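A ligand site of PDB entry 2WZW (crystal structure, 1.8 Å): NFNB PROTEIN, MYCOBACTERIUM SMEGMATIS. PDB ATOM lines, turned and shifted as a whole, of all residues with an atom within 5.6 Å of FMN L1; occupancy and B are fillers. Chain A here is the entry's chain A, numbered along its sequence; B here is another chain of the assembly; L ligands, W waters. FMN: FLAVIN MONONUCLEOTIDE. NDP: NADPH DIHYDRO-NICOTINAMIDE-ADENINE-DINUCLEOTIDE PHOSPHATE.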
ATOM      1  N   ARG A  26     -11.535  -7.894  33.289  1.00  0.00           N
ATOM      2  CA  ARG A  26     -12.151  -7.673  31.987  1.00  0.00           C
ATOM      3  C   ARG A  26     -11.291  -8.385  30.928  1.00  0.00           C
ATOM      4  O   ARG A  26     -10.077  -8.207  30.907  1.00  0.00           O
ATOM      5  CB  ARG A  26     -12.254  -6.164  31.670  1.00  0.00           C
ATOM      6  CG  ARG A  26     -12.921  -5.837  30.309  1.00  0.00           C
ATOM      7  CD  ARG A  26     -12.147  -4.814  29.454  1.00  0.00           C
ATOM      8  NE  ARG A  26     -10.717  -5.151  29.325  1.00  0.00           N
ATOM      9  CZ  ARG A  26     -10.203  -6.007  28.446  1.00  0.00           C
ATOM     10  NH1 ARG A  26     -10.999  -6.616  27.567  1.00  0.00           N
ATOM     11  NH2 ARG A  26      -8.909  -6.279  28.461  1.00  0.00           N
ATOM     12  N   ARG A  27     -11.941  -9.185  30.081  1.00  0.00           N
ATOM     13  CA  ARG A  27     -11.307  -9.931  28.979  1.00  0.00           C
ATOM     14  C   ARG A  27     -12.234  -9.925  27.779  1.00  0.00           C
ATOM     15  O   ARG A  27     -13.436  -9.707  27.952  1.00  0.00           O
ATOM     16  CB  ARG A  27     -11.018 -11.389  29.387  1.00  0.00           C
ATOM     17  CG  ARG A  27      -9.759 -11.545  30.221  1.00  0.00           C
ATOM     18  CD  ARG A  27      -9.536 -12.998  30.634  1.00  0.00           C
ATOM     19  NE  ARG A  27     -10.376 -13.371  31.780  1.00  0.00           N
ATOM     20  CZ  ARG A  27     -10.055 -13.144  33.053  1.00  0.00           C
ATOM     21  NH1 ARG A  27      -8.907 -12.554  33.368  1.00  0.00           N
ATOM     22  NH2 ARG A  27     -10.885 -13.505  34.025  1.00  0.00           N
ATOM     23  N   ALA A  28     -11.698 -10.130  26.561  1.00  0.00           N
ATOM     24  CA  ALA A  28     -12.510 -10.202  25.353  1.00  0.00           C
ATOM     25  C   ALA A  28     -13.138 -11.595  25.374  1.00  0.00           C
ATOM     26  O   ALA A  28     -12.442 -12.612  25.235  1.00  0.00           O
ATOM     27  CB  ALA A  28     -11.645 -10.025  24.101  1.00  0.00           C
ATOM     28  N   ARG A  30     -15.690 -14.386  23.868  1.00  0.00           N
ATOM     29  CA  ARG A  30     -16.151 -14.777  22.527  1.00  0.00           C
ATOM     30  C   ARG A  30     -17.147 -15.945  22.475  1.00  0.00           C
ATOM     31  O   ARG A  30     -17.279 -16.604  21.437  1.00  0.00           O
ATOM     32  CB  ARG A  30     -14.940 -14.999  21.597  1.00  0.00           C
ATOM     33  CG  ARG A  30     -14.053 -13.755  21.469  1.00  0.00           C
ATOM     34  CD  ARG A  30     -12.824 -14.015  20.620  1.00  0.00           C
ATOM     35  NE  ARG A  30     -12.019 -12.805  20.454  1.00  0.00           N
ATOM     36  CZ  ARG A  30     -10.991 -12.456  21.233  1.00  0.00           C
ATOM     37  NH1 ARG A  30     -10.639 -13.226  22.250  1.00  0.00           N
ATOM     38  NH2 ARG A  30     -10.321 -11.342  21.001  1.00  0.00           N
ATOM     39  N   PHE A 109      -0.981 -12.542  19.411  1.00  0.00           N
ATOM     40  CA  PHE A 109      -2.392 -12.620  19.843  1.00  0.00           C
ATOM     41  C   PHE A 109      -3.157 -13.641  18.954  1.00  0.00           C
ATOM     42  O   PHE A 109      -3.878 -14.495  19.476  1.00  0.00           O
ATOM     43  CB  PHE A 109      -3.048 -11.214  19.784  1.00  0.00           C
ATOM     44  CG  PHE A 109      -4.534 -11.261  19.493  1.00  0.00           C
ATOM     45  CD1 PHE A 109      -5.439 -11.705  20.448  1.00  0.00           C
ATOM     46  CD2 PHE A 109      -5.022 -10.887  18.243  1.00  0.00           C
ATOM     47  CE1 PHE A 109      -6.806 -11.787  20.160  1.00  0.00           C
ATOM     48  CE2 PHE A 109      -6.397 -10.958  17.959  1.00  0.00           C
ATOM     49  CZ  PHE A 109      -7.279 -11.397  18.919  1.00  0.00           C
ATOM     50  N   LEU A 113      -5.279 -16.888  20.022  1.00  0.00           N
ATOM     51  CA  LEU A 113      -6.709 -16.997  19.758  1.00  0.00           C
ATOM     52  C   LEU A 113      -7.057 -18.202  18.864  1.00  0.00           C
ATOM     53  O   LEU A 113      -7.896 -19.029  19.245  1.00  0.00           O
ATOM     54  CB  LEU A 113      -7.257 -15.698  19.152  1.00  0.00           C
ATOM     55  CG  LEU A 113      -8.733 -15.727  18.694  1.00  0.00           C
ATOM     56  CD1 LEU A 113      -9.679 -15.954  19.880  1.00  0.00           C
ATOM     57  CD2 LEU A 113      -9.087 -14.480  17.920  1.00  0.00           C
ATOM     58  N   TYR A 130     -16.177 -19.188  11.723  1.00  0.00           N
ATOM     59  CA  TYR A 130     -15.846 -18.389  12.903  1.00  0.00           C
ATOM     60  C   TYR A 130     -16.241 -16.902  12.716  1.00  0.00           C
ATOM     61  O   TYR A 130     -16.815 -16.296  13.635  1.00  0.00           O
ATOM     62  CB  TYR A 130     -14.368 -18.554  13.301  1.00  0.00           C
ATOM     63  CG  TYR A 130     -13.933 -17.562  14.363  1.00  0.00           C
ATOM     64  CD1 TYR A 130     -14.387 -17.683  15.677  1.00  0.00           C
ATOM     65  CD2 TYR A 130     -13.119 -16.486  14.045  1.00  0.00           C
ATOM     66  CE1 TYR A 130     -14.054 -16.732  16.638  1.00  0.00           C
ATOM     67  CE2 TYR A 130     -12.754 -15.541  15.007  1.00  0.00           C
ATOM     68  CZ  TYR A 130     -13.229 -15.669  16.302  1.00  0.00           C
ATOM     69  OH  TYR A 130     -12.854 -14.744  17.239  1.00  0.00           O
ATOM     70  N   TYR A 138     -21.130 -13.411  18.718  1.00  0.00           N
ATOM     71  CA  TYR A 138     -20.725 -14.564  19.532  1.00  0.00           C
ATOM     72  C   TYR A 138     -21.890 -15.122  20.400  1.00  0.00           C
ATOM     73  O   TYR A 138     -21.660 -15.709  21.449  1.00  0.00           O
ATOM     74  CB  TYR A 138     -19.505 -14.204  20.399  1.00  0.00           C
ATOM     75  CG  TYR A 138     -18.287 -13.753  19.620  1.00  0.00           C
ATOM     76  CD1 TYR A 138     -17.577 -14.646  18.822  1.00  0.00           C
ATOM     77  CD2 TYR A 138     -17.780 -12.463  19.755  1.00  0.00           C
ATOM     78  CE1 TYR A 138     -16.404 -14.268  18.171  1.00  0.00           C
ATOM     79  CE2 TYR A 138     -16.625 -12.062  19.084  1.00  0.00           C
ATOM     80  CZ  TYR A 138     -15.936 -12.969  18.303  1.00  0.00           C
ATOM     81  OH  TYR A 138     -14.791 -12.587  17.638  1.00  0.00           O
ATOM     82  N   MET A 168     -16.802  -0.785  29.292  1.00  0.00           N
ATOM     83  CA  MET A 168     -16.414  -2.178  29.527  1.00  0.00           C
ATOM     84  C   MET A 168     -16.115  -2.449  31.006  1.00  0.00           C
ATOM     85  O   MET A 168     -16.443  -3.538  31.492  1.00  0.00           O
ATOM     86  CB  MET A 168     -15.253  -2.609  28.620  1.00  0.00           C
ATOM     87  CG  MET A 168     -15.676  -2.709  27.142  1.00  0.00           C
ATOM     88  SD  MET A 168     -14.249  -3.391  25.988  1.00  0.00           S
ATOM     89  CE  MET A 168     -13.095  -1.784  25.858  1.00  0.00           C
ATOM     90  N   CYS A 179     -17.067  -8.074  24.459  1.00  0.00           N
ATOM     91  CA  CYS A 179     -16.047  -8.208  23.422  1.00  0.00           C
ATOM     92  C   CYS A 179     -16.107  -6.986  22.523  1.00  0.00           C
ATOM     93  O   CYS A 179     -17.108  -6.816  21.793  1.00  0.00           O
ATOM     94  CB  CYS A 179     -16.169  -9.486  22.611  1.00  0.00           C
ATOM     95  SG  CYS A 179     -14.734  -9.788  21.523  1.00  0.00           S
ATOM     96  N   PRO A 180     -15.057  -6.133  22.548  1.00  0.00           N
ATOM     97  CA  PRO A 180     -15.033  -5.000  21.612  1.00  0.00           C
ATOM     98  C   PRO A 180     -14.769  -5.582  20.237  1.00  0.00           C
ATOM     99  O   PRO A 180     -14.000  -6.568  20.127  1.00  0.00           O
ATOM    100  CB  PRO A 180     -13.860  -4.137  22.088  1.00  0.00           C
ATOM    101  CG  PRO A 180     -12.979  -5.054  22.881  1.00  0.00           C
ATOM    102  CD  PRO A 180     -13.817  -6.211  23.362  1.00  0.00           C
ATOM    103  N   GLN A 181     -15.486  -5.096  19.213  1.00  0.00           N
ATOM    104  CA  GLN A 181     -15.312  -5.670  17.889  1.00  0.00           C
ATOM    105  C   GLN A 181     -15.152  -4.610  16.803  1.00  0.00           C
ATOM    106  O   GLN A 181     -16.147  -3.998  16.394  1.00  0.00           O
ATOM    107  CB  GLN A 181     -16.500  -6.604  17.519  1.00  0.00           C
ATOM    108  CG  GLN A 181     -16.599  -7.881  18.341  1.00  0.00           C
ATOM    109  CD  GLN A 181     -17.839  -8.655  17.957  1.00  0.00           C
ATOM    110  OE1 GLN A 181     -18.898  -8.459  18.510  1.00  0.00           O
ATOM    111  NE2 GLN A 181     -17.736  -9.536  16.983  1.00  0.00           N
ATOM    112  N   ALA A 182     -13.936  -4.481  16.262  1.00  0.00           N
ATOM    113  CA  ALA A 182     -13.682  -3.623  15.095  1.00  0.00           C
ATOM    114  C   ALA A 182     -14.403  -4.256  13.877  1.00  0.00           C
ATOM    115  O   ALA A 182     -14.819  -3.536  12.967  1.00  0.00           O
ATOM    116  CB  ALA A 182     -12.190  -3.525  14.805  1.00  0.00           C
ATOM    117  N   LEU A 183     -14.533  -5.606  13.860  1.00  0.00           N
ATOM    118  CA  LEU A 183     -15.192  -6.311  12.753  1.00  0.00           C
ATOM    119  C   LEU A 183     -16.543  -5.701  12.332  1.00  0.00           C
ATOM    120  O   LEU A 183     -16.820  -5.563  11.134  1.00  0.00           O
ATOM    121  CB  LEU A 183     -15.363  -7.805  13.069  1.00  0.00           C
ATOM    122  CG  LEU A 183     -16.178  -8.613  12.037  1.00  0.00           C
ATOM    123  CD1 LEU A 183     -15.412  -8.770  10.716  1.00  0.00           C
ATOM    124  CD2 LEU A 183     -16.599  -9.947  12.606  1.00  0.00           C
ATOM    125  N   LEU A 184     -17.377  -5.355  13.303  1.00  0.00           N
ATOM    126  CA  LEU A 184     -18.709  -4.799  13.054  1.00  0.00           C
ATOM    127  C   LEU A 184     -18.684  -3.459  12.309  1.00  0.00           C
ATOM    128  O   LEU A 184     -19.628  -3.145  11.592  1.00  0.00           O
ATOM    129  CB  LEU A 184     -19.495  -4.687  14.382  1.00  0.00           C
ATOM    130  CG  LEU A 184     -19.631  -6.011  15.186  1.00  0.00           C
ATOM    131  CD1 LEU A 184     -20.336  -5.772  16.498  1.00  0.00           C
ATOM    132  CD2 LEU A 184     -20.353  -7.103  14.395  1.00  0.00           C
ATOM    133  N   MET A 204     -16.791   1.059  16.243  1.00  0.00           N
ATOM    134  CA  MET A 204     -16.742  -0.328  16.732  1.00  0.00           C
ATOM    135  C   MET A 204     -18.088  -0.710  17.313  1.00  0.00           C
ATOM    136  O   MET A 204     -18.917   0.171  17.558  1.00  0.00           O
ATOM    137  CB  MET A 204     -15.663  -0.484  17.845  1.00  0.00           C
ATOM    138  CG  MET A 204     -16.109   0.067  19.224  1.00  0.00           C
ATOM    139  SD  MET A 204     -14.816  -0.217  20.657  1.00  0.00           S
ATOM    140  CE  MET A 204     -13.740   1.385  20.399  1.00  0.00           C
ATOM    141  N   ILE A 222      -4.762 -13.588  27.208  1.00  0.00           N
ATOM    142  CA  ILE A 222      -3.834 -12.822  26.379  1.00  0.00           C
ATOM    143  C   ILE A 222      -2.884 -11.995  27.237  1.00  0.00           C
ATOM    144  O   ILE A 222      -3.353 -11.235  28.092  1.00  0.00           O
ATOM    145  CB  ILE A 222      -4.647 -11.965  25.375  1.00  0.00           C
ATOM    146  CG1 ILE A 222      -5.569 -12.858  24.479  1.00  0.00           C
ATOM    147  CG2 ILE A 222      -3.767 -11.049  24.541  1.00  0.00           C
ATOM    148  CD1 ILE A 222      -4.864 -13.956  23.591  1.00  0.00           C
ATOM    149  N   ARG A 224       0.393  -9.220  28.172  1.00  0.00           N
ATOM    150  CA  ARG A 224       0.730  -7.842  27.849  1.00  0.00           C
ATOM    151  C   ARG A 224       2.256  -7.759  27.816  1.00  0.00           C
ATOM    152  O   ARG A 224       2.929  -8.580  28.455  1.00  0.00           O
ATOM    153  CB  ARG A 224       0.155  -6.845  28.881  1.00  0.00           C
ATOM    154  CG  ARG A 224      -1.382  -6.747  28.870  1.00  0.00           C
ATOM    155  CD  ARG A 224      -1.983  -6.202  27.561  1.00  0.00           C
ATOM    156  NE  ARG A 224      -3.421  -5.923  27.708  1.00  0.00           N
ATOM    157  CZ  ARG A 224      -4.382  -6.837  27.558  1.00  0.00           C
ATOM    158  NH1 ARG A 224      -4.069  -8.099  27.258  1.00  0.00           N
ATOM    159  NH2 ARG A 224      -5.651  -6.492  27.725  1.00  0.00           N
ATOM    160  N   HIS B  51      -2.789  -3.314  31.259  1.00  0.00           N
ATOM    161  CA  HIS B  51      -3.854  -4.300  31.011  1.00  0.00           C
ATOM    162  C   HIS B  51      -5.022  -3.776  30.168  1.00  0.00           C
ATOM    163  O   HIS B  51      -5.981  -4.506  29.927  1.00  0.00           O
ATOM    164  CB  HIS B  51      -4.332  -4.994  32.305  1.00  0.00           C
ATOM    165  CG  HIS B  51      -3.295  -5.908  32.865  1.00  0.00           C
ATOM    166  ND1 HIS B  51      -3.207  -7.221  32.450  1.00  0.00           N
ATOM    167  CD2 HIS B  51      -2.260  -5.639  33.697  1.00  0.00           C
ATOM    168  CE1 HIS B  51      -2.167  -7.730  33.093  1.00  0.00           C
ATOM    169  NE2 HIS B  51      -1.561  -6.810  33.837  1.00  0.00           N
ATOM    170  N   PRO B  53      -7.197  -3.120  26.924  1.00  0.00           N
ATOM    171  CA  PRO B  53      -7.265  -3.861  25.654  1.00  0.00           C
ATOM    172  C   PRO B  53      -6.905  -2.917  24.482  1.00  0.00           C
ATOM    173  O   PRO B  53      -6.783  -1.709  24.665  1.00  0.00           O
ATOM    174  CB  PRO B  53      -8.753  -4.275  25.576  1.00  0.00           C
ATOM    175  CG  PRO B  53      -9.475  -3.101  26.241  1.00  0.00           C
ATOM    176  CD  PRO B  53      -8.538  -2.675  27.378  1.00  0.00           C
ATOM    177  N   SER B  54      -6.689  -3.493  23.285  1.00  0.00           N
ATOM    178  CA  SER B  54      -6.360  -2.721  22.079  1.00  0.00           C
ATOM    179  C   SER B  54      -6.626  -3.608  20.894  1.00  0.00           C
ATOM    180  O   SER B  54      -6.693  -4.839  21.077  1.00  0.00           O
ATOM    181  CB  SER B  54      -4.884  -2.294  22.102  1.00  0.00           C
ATOM    182  OG  SER B  54      -4.015  -3.406  22.284  1.00  0.00           O
ATOM    183  N   ASN B  55      -6.711  -3.021  19.689  1.00  0.00           N
ATOM    184  CA  ASN B  55      -6.907  -3.807  18.444  1.00  0.00           C
ATOM    185  C   ASN B  55      -5.785  -4.835  18.334  1.00  0.00           C
ATOM    186  O   ASN B  55      -4.609  -4.442  18.413  1.00  0.00           O
ATOM    187  CB  ASN B  55      -6.869  -2.888  17.220  1.00  0.00           C
ATOM    188  CG  ASN B  55      -8.071  -2.003  17.084  1.00  0.00           C
ATOM    189  OD1 ASN B  55      -9.081  -2.390  16.503  1.00  0.00           O
ATOM    190  ND2 ASN B  55      -7.993  -0.776  17.576  1.00  0.00           N
ATOM    191  N   SER B  56      -6.128  -6.133  18.239  1.00  0.00           N
ATOM    192  CA  SER B  56      -5.164  -7.241  18.092  1.00  0.00           C
ATOM    193  C   SER B  56      -4.089  -7.272  19.206  1.00  0.00           C
ATOM    194  O   SER B  56      -2.988  -7.777  18.958  1.00  0.00           O
ATOM    195  CB  SER B  56      -4.447  -7.124  16.754  1.00  0.00           C
ATOM    196  OG  SER B  56      -5.294  -7.419  15.654  1.00  0.00           O
ATOM    197  N   ASN B  57      -4.364  -6.686  20.388  1.00  0.00           N
ATOM    198  CA  ASN B  57      -3.397  -6.602  21.501  1.00  0.00           C
ATOM    199  C   ASN B  57      -2.091  -5.858  21.086  1.00  0.00           C
ATOM    200  O   ASN B  57      -1.006  -6.125  21.613  1.00  0.00           O
ATOM    201  CB  ASN B  57      -3.116  -8.010  22.092  1.00  0.00           C
ATOM    202  CG  ASN B  57      -2.477  -7.972  23.467  1.00  0.00           C
ATOM    203  OD1 ASN B  57      -2.914  -7.225  24.346  1.00  0.00           O
ATOM    204  ND2 ASN B  57      -1.435  -8.789  23.675  1.00  0.00           N
ATOM    205  N   ASP B 159      -7.503   3.306  20.811  1.00  0.00           N
ATOM    206  CA  ASP B 159      -6.752   2.490  21.782  1.00  0.00           C
ATOM    207  C   ASP B 159      -5.936   3.336  22.745  1.00  0.00           C
ATOM    208  O   ASP B 159      -5.813   2.978  23.921  1.00  0.00           O
ATOM    209  CB  ASP B 159      -5.852   1.494  21.032  1.00  0.00           C
ATOM    210  CG  ASP B 159      -6.635   0.411  20.313  1.00  0.00           C
ATOM    211  OD1 ASP B 159      -7.848   0.257  20.602  1.00  0.00           O
ATOM    212  OD2 ASP B 159      -6.034  -0.305  19.492  1.00  0.00           O
ATOM    213  N   ILE B 162      -8.456   4.314  25.317  1.00  0.00           N
ATOM    214  CA  ILE B 162      -8.709   3.155  26.186  1.00  0.00           C
ATOM    215  C   ILE B 162      -7.611   3.099  27.264  1.00  0.00           C
ATOM    216  O   ILE B 162      -7.901   3.024  28.459  1.00  0.00           O
ATOM    217  CB  ILE B 162      -8.770   1.852  25.362  1.00  0.00           C
ATOM    218  CG1 ILE B 162     -10.043   1.798  24.502  1.00  0.00           C
ATOM    219  CG2 ILE B 162      -8.666   0.611  26.274  1.00  0.00           C
ATOM    220  CD1 ILE B 162     -10.135   0.515  23.618  1.00  0.00           C
HETATM  221  N1  FMN L   1     -11.533  -9.058  19.098  1.00  0.00           N
HETATM  222  C2  FMN L   1     -12.210  -9.786  18.179  1.00  0.00           C
HETATM  223  O2  FMN L   1     -12.346 -11.110  18.384  1.00  0.00           O
HETATM  224  N3  FMN L   1     -12.747  -9.214  17.079  1.00  0.00           N
HETATM  225  C4  FMN L   1     -12.586  -7.893  16.859  1.00  0.00           C
HETATM  226  O4  FMN L   1     -13.105  -7.329  15.764  1.00  0.00           O
HETATM  227  C4A FMN L   1     -11.890  -7.112  17.792  1.00  0.00           C
HETATM  228  N5  FMN L   1     -11.709  -5.730  17.592  1.00  0.00           N
HETATM  229  C5A FMN L   1     -11.265  -4.941  18.676  1.00  0.00           C
HETATM  230  C6  FMN L   1     -11.363  -3.540  18.619  1.00  0.00           C
HETATM  231  C7  FMN L   1     -10.913  -2.769  19.692  1.00  0.00           C
HETATM  232  C7M FMN L   1     -10.984  -1.235  19.621  1.00  0.00           C
HETATM  233  C8  FMN L   1     -10.403  -3.398  20.842  1.00  0.00           C
HETATM  234  C8M FMN L   1      -9.946  -2.569  22.057  1.00  0.00           C
HETATM  235  C9  FMN L   1     -10.309  -4.782  20.896  1.00  0.00           C
HETATM  236  C9A FMN L   1     -10.777  -5.561  19.834  1.00  0.00           C
HETATM  237  N10 FMN L   1     -10.706  -6.988  19.909  1.00  0.00           N
HETATM  238  C10 FMN L   1     -11.363  -7.733  18.931  1.00  0.00           C
HETATM  239  C1' FMN L   1     -10.401  -7.645  21.225  1.00  0.00           C
HETATM  240  C2' FMN L   1      -8.914  -8.029  21.385  1.00  0.00           C
HETATM  241  O2' FMN L   1      -8.264  -8.497  20.441  1.00  0.00           O
HETATM  242  C3' FMN L   1      -8.347  -7.968  22.807  1.00  0.00           C
HETATM  243  O3' FMN L   1      -8.825  -6.835  23.578  1.00  0.00           O
HETATM  244  C4' FMN L   1      -6.816  -8.109  22.894  1.00  0.00           C
HETATM  245  O4' FMN L   1      -6.446  -9.364  22.284  1.00  0.00           O
HETATM  246  C5' FMN L   1      -6.427  -8.164  24.380  1.00  0.00           C
HETATM  247  O5' FMN L   1      -7.069  -9.320  25.002  1.00  0.00           O
HETATM  248  P   FMN L   1      -8.047  -9.173  26.267  1.00  0.00           P
HETATM  249  O1P FMN L   1      -9.103  -8.004  25.998  1.00  0.00           O
HETATM  250  O2P FMN L   1      -8.840 -10.542  26.349  1.00  0.00           O
HETATM  251  O3P FMN L   1      -7.294  -8.868  27.518  1.00  0.00           O
HETATM  252  PA  NDP L   2      -7.386 -11.121  12.780  1.00  0.00           P
HETATM  253  O1A NDP L   2      -7.854 -12.181  13.727  1.00  0.00           O
HETATM  254  O2A NDP L   2      -7.893 -11.108  11.373  1.00  0.00           O
HETATM  255  O5B NDP L   2      -5.781 -11.394  12.643  1.00  0.00           O
HETATM  256  C5B NDP L   2      -4.977 -11.280  13.824  1.00  0.00           C
HETATM  257  C4B NDP L   2      -3.631 -12.012  13.642  1.00  0.00           C
HETATM  258  O4B NDP L   2      -3.877 -13.428  13.582  1.00  0.00           O
HETATM  259  C3B NDP L   2      -2.894 -11.634  12.347  1.00  0.00           C
HETATM  260  O3B NDP L   2      -1.451 -11.623  12.580  1.00  0.00           O
HETATM  261  C2B NDP L   2      -3.312 -12.771  11.407  1.00  0.00           C
HETATM  262  O2B NDP L   2      -2.444 -12.864  10.294  1.00  0.00           O
HETATM  263  C1B NDP L   2      -3.280 -13.959  12.376  1.00  0.00           C
HETATM  264  N9A NDP L   2      -4.034 -15.160  12.056  1.00  0.00           N
HETATM  265  C8A NDP L   2      -5.153 -15.263  11.252  1.00  0.00           C
HETATM  266  N7A NDP L   2      -5.604 -16.516  11.170  1.00  0.00           N
HETATM  267  C5A NDP L   2      -4.742 -17.249  11.947  1.00  0.00           C
HETATM  268  C6A NDP L   2      -4.663 -18.633  12.297  1.00  0.00           C
HETATM  269  N6A NDP L   2      -5.565 -19.573  11.857  1.00  0.00           N
HETATM  270  N1A NDP L   2      -3.646 -19.063  13.139  1.00  0.00           N
HETATM  271  C2A NDP L   2      -2.744 -18.139  13.595  1.00  0.00           C
HETATM  272  N3A NDP L   2      -2.733 -16.800  13.337  1.00  0.00           N
HETATM  273  C4A NDP L   2      -3.752 -16.415  12.514  1.00  0.00           C
HETATM  274  O3  NDP L   2      -7.375  -9.651  13.436  1.00  0.00           O
HETATM  275  PN  NDP L   2      -7.110  -8.221  12.732  1.00  0.00           P
HETATM  276  O1N NDP L   2      -6.813  -7.093  13.689  1.00  0.00           O
HETATM  277  O2N NDP L   2      -6.264  -8.457  11.483  1.00  0.00           O
HETATM  278  O5D NDP L   2      -8.590  -7.886  12.156  1.00  0.00           O
HETATM  279  C5D NDP L   2      -9.567  -7.295  13.010  1.00  0.00           C
HETATM  280  C4D NDP L   2     -11.021  -7.732  12.774  1.00  0.00           C
HETATM  281  O4D NDP L   2     -11.516  -6.840  11.769  1.00  0.00           O
HETATM  282  C3D NDP L   2     -11.223  -9.160  12.222  1.00  0.00           C
HETATM  283  O3D NDP L   2     -12.523  -9.684  12.506  1.00  0.00           O
HETATM  284  C2D NDP L   2     -10.976  -8.982  10.735  1.00  0.00           C
HETATM  285  O2D NDP L   2     -11.625 -10.022   9.964  1.00  0.00           O
HETATM  286  C1D NDP L   2     -11.561  -7.575  10.504  1.00  0.00           C
HETATM  287  N1N NDP L   2     -10.877  -6.837   9.422  1.00  0.00           N
HETATM  288  C2N NDP L   2     -11.508  -6.764   8.147  1.00  0.00           C
HETATM  289  C3N NDP L   2     -10.968  -6.095   7.075  1.00  0.00           C
HETATM  290  C7N NDP L   2     -11.727  -6.060   5.758  1.00  0.00           C
HETATM  291  O7N NDP L   2     -12.833  -6.613   5.588  1.00  0.00           O
HETATM  292  N7N NDP L   2     -11.147  -5.378   4.724  1.00  0.00           N
HETATM  293  C4N NDP L   2      -9.608  -5.396   7.240  1.00  0.00           C
HETATM  294  C5N NDP L   2      -8.985  -5.520   8.628  1.00  0.00           C
HETATM  295  C6N NDP L   2      -9.620  -6.210   9.606  1.00  0.00           C
HETATM  296  P2B NDP L   2      -2.908 -12.232   8.869  1.00  0.00           P
HETATM  297  O1X NDP L   2      -2.040 -11.025   8.595  1.00  0.00           O
HETATM  298  O2X NDP L   2      -2.564 -13.408   7.990  1.00  0.00           O
HETATM  299  O3X NDP L   2      -4.379 -11.870   8.862  1.00  0.00           O
HETATM  300  O   HOH W   1      -5.711 -10.166  28.991  1.00  0.00           O
HETATM  301  O   HOH W   2      -9.943   1.679  18.190  1.00  0.00           O
HETATM  302  O   HOH W   3      -8.357 -11.388  23.241  1.00  0.00           O
HETATM  303  O   HOH W   4     -11.743 -12.635  16.222  1.00  0.00           O
HETATM  304  O   HOH W   5      -7.549 -12.653  27.676  1.00  0.00           O
HETATM  305  O   HOH W   6     -10.374   1.941  20.632  1.00  0.00           O
HETATM  306  O   HOH W   7     -14.917 -10.455  15.908  1.00  0.00           O
HETATM  307  O   HOH W   8      -9.808 -12.943  25.502  1.00  0.00           O
HETATM  308  O   HOH W   9      -9.085  -5.023  15.785  1.00  0.00           O
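NE of Arg 30 is in hydrogen-bond range of O2 of FMN L1 (2.7 Å).
NH1 of Arg 26 lies within salt-bridge range of O1P of FMN L1 (2.8 Å).
A nitrogen (N5) of FMN L1 lies within hydrogen-bond range of the backbone NH (N) of Ala 182 (2.9 Å).
An oxygen (O2P) of FMN L1 lies within hydrogen-bond range of the backbone NH of Ala 28.
An oxygen (O3P) of FMN L1 lies within salt-bridge range of the guanidinium group (NH2) of Arg 224, 2.9 Å away.
An oxygen (O4) of FMN L1 lies within hydrogen-bond range of the backbone NH (N) of Leu 183.
An oxygen (O2) of FMN L1 sits at hydrogen-bond distance from the side-chain hydroxyl (OH) of Tyr 138, 3.0 Å away.
OG of Ser 56 of chain B is in hydrogen-bond range of O1N of NDP L2, 2.5 Å away.
The side-chain amide oxygen (OD1) of Asn 57 of chain B sits at hydrogen-bond distance from the guanidinium group (NH1) of Arg 224 (3.3 Å).
NH1 of Arg 224 lies within hydrogen-bond range of O of Ile 222 (3.3 Å).
The guanidinium group of Arg 224 lies within hydrogen-bond range of the backbone carbonyl oxygen of His 51 of chain B (3.0 Å).
The side-chain hydroxyl (OH) of Tyr 138 lies within hydrogen-bond range of the side-chain hydroxyl (OH) of Tyr 130.
The side-chain carboxylate of Asp 159 of chain B sits at hydrogen-bond distance from the side-chain amide nitrogen of Asn 55 of chain B (2.8 Å).
The backbone carbonyl oxygen of Pro 180 sits close to a nitrogen (N10) of FMN L1.
Merely in contact with FMN L1: Arg 27 (3.7 Å), Phe 109 (3.1 Å), Tyr 130 (3.8 Å), Gln 181 (3.5 Å), Met 204 (3.9 Å), Ile 222 (3.6 Å), Pro 53 of chain B (3.2 Å), Ser 54 of chain B (3.6 Å), Asn 55 of chain B (3.3 Å), Ser 56 of chain B (3.9 Å), Asn 57 of chain B (3.6 Å), Asp 159 of chain B (3.6 Å) and Ile 162 of chain B (3.5 Å).
Hydrophobic or aromatic side chains that line FMN L1: Ala 28, Phe 109, Pro 180, Ala 182, Leu 183, Met 204, Ile 222, Pro 53 of chain B and Ile 162 of chain B.
21 residues have an atom within 4 Å of FMN L1: Arg 26, Arg 27, Ala 28, Arg 30, Phe 109, Tyr 130, Tyr 138, Pro 180, Gln 181, Ala 182, Leu 183, Met 204, Ile 222, Arg 224, Pro 53 of chain B, Ser 54 of chain B, Asn 55 of chain B, Ser 56 of chain B, Asn 57 of chain B, Asp 159 of chain B and Ile 162 of chain B.
Along chain A the residues within 4 Å of FMN L1 span positions 26 to 224.
The nearest printed residue that does not touch FMN L1 is Cys 179 (4.1 Å).
Water W1 lies within hydrogen-bond range of O3P of FMN L1 (2.5 Å), O of Ile 222 (2.7 Å) and NH1 of Arg 224 (3.2 Å).
Water W4 lies within hydrogen-bond range of OH of Tyr 130 (2.6 Å), O2 of FMN L1 (2.7 Å) and OH of Tyr 138 (3.4 Å).
Water W5 bridges O2P of FMN L1 (2.8 Å) and N of Ile 222 (3.0 Å).
Water W3 lies within hydrogen-bond range of O4' of FMN L1 and NH2 of Arg 30.
Water W9 bridges OD1 of Asn 55 of chain B (2.7 Å) and N5 of FMN L1 (3.3 Å).
Water W2 lies within hydrogen-bond range of ND2 of Asn 55 of chain B and OD1 of Asp 159 of chain B.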
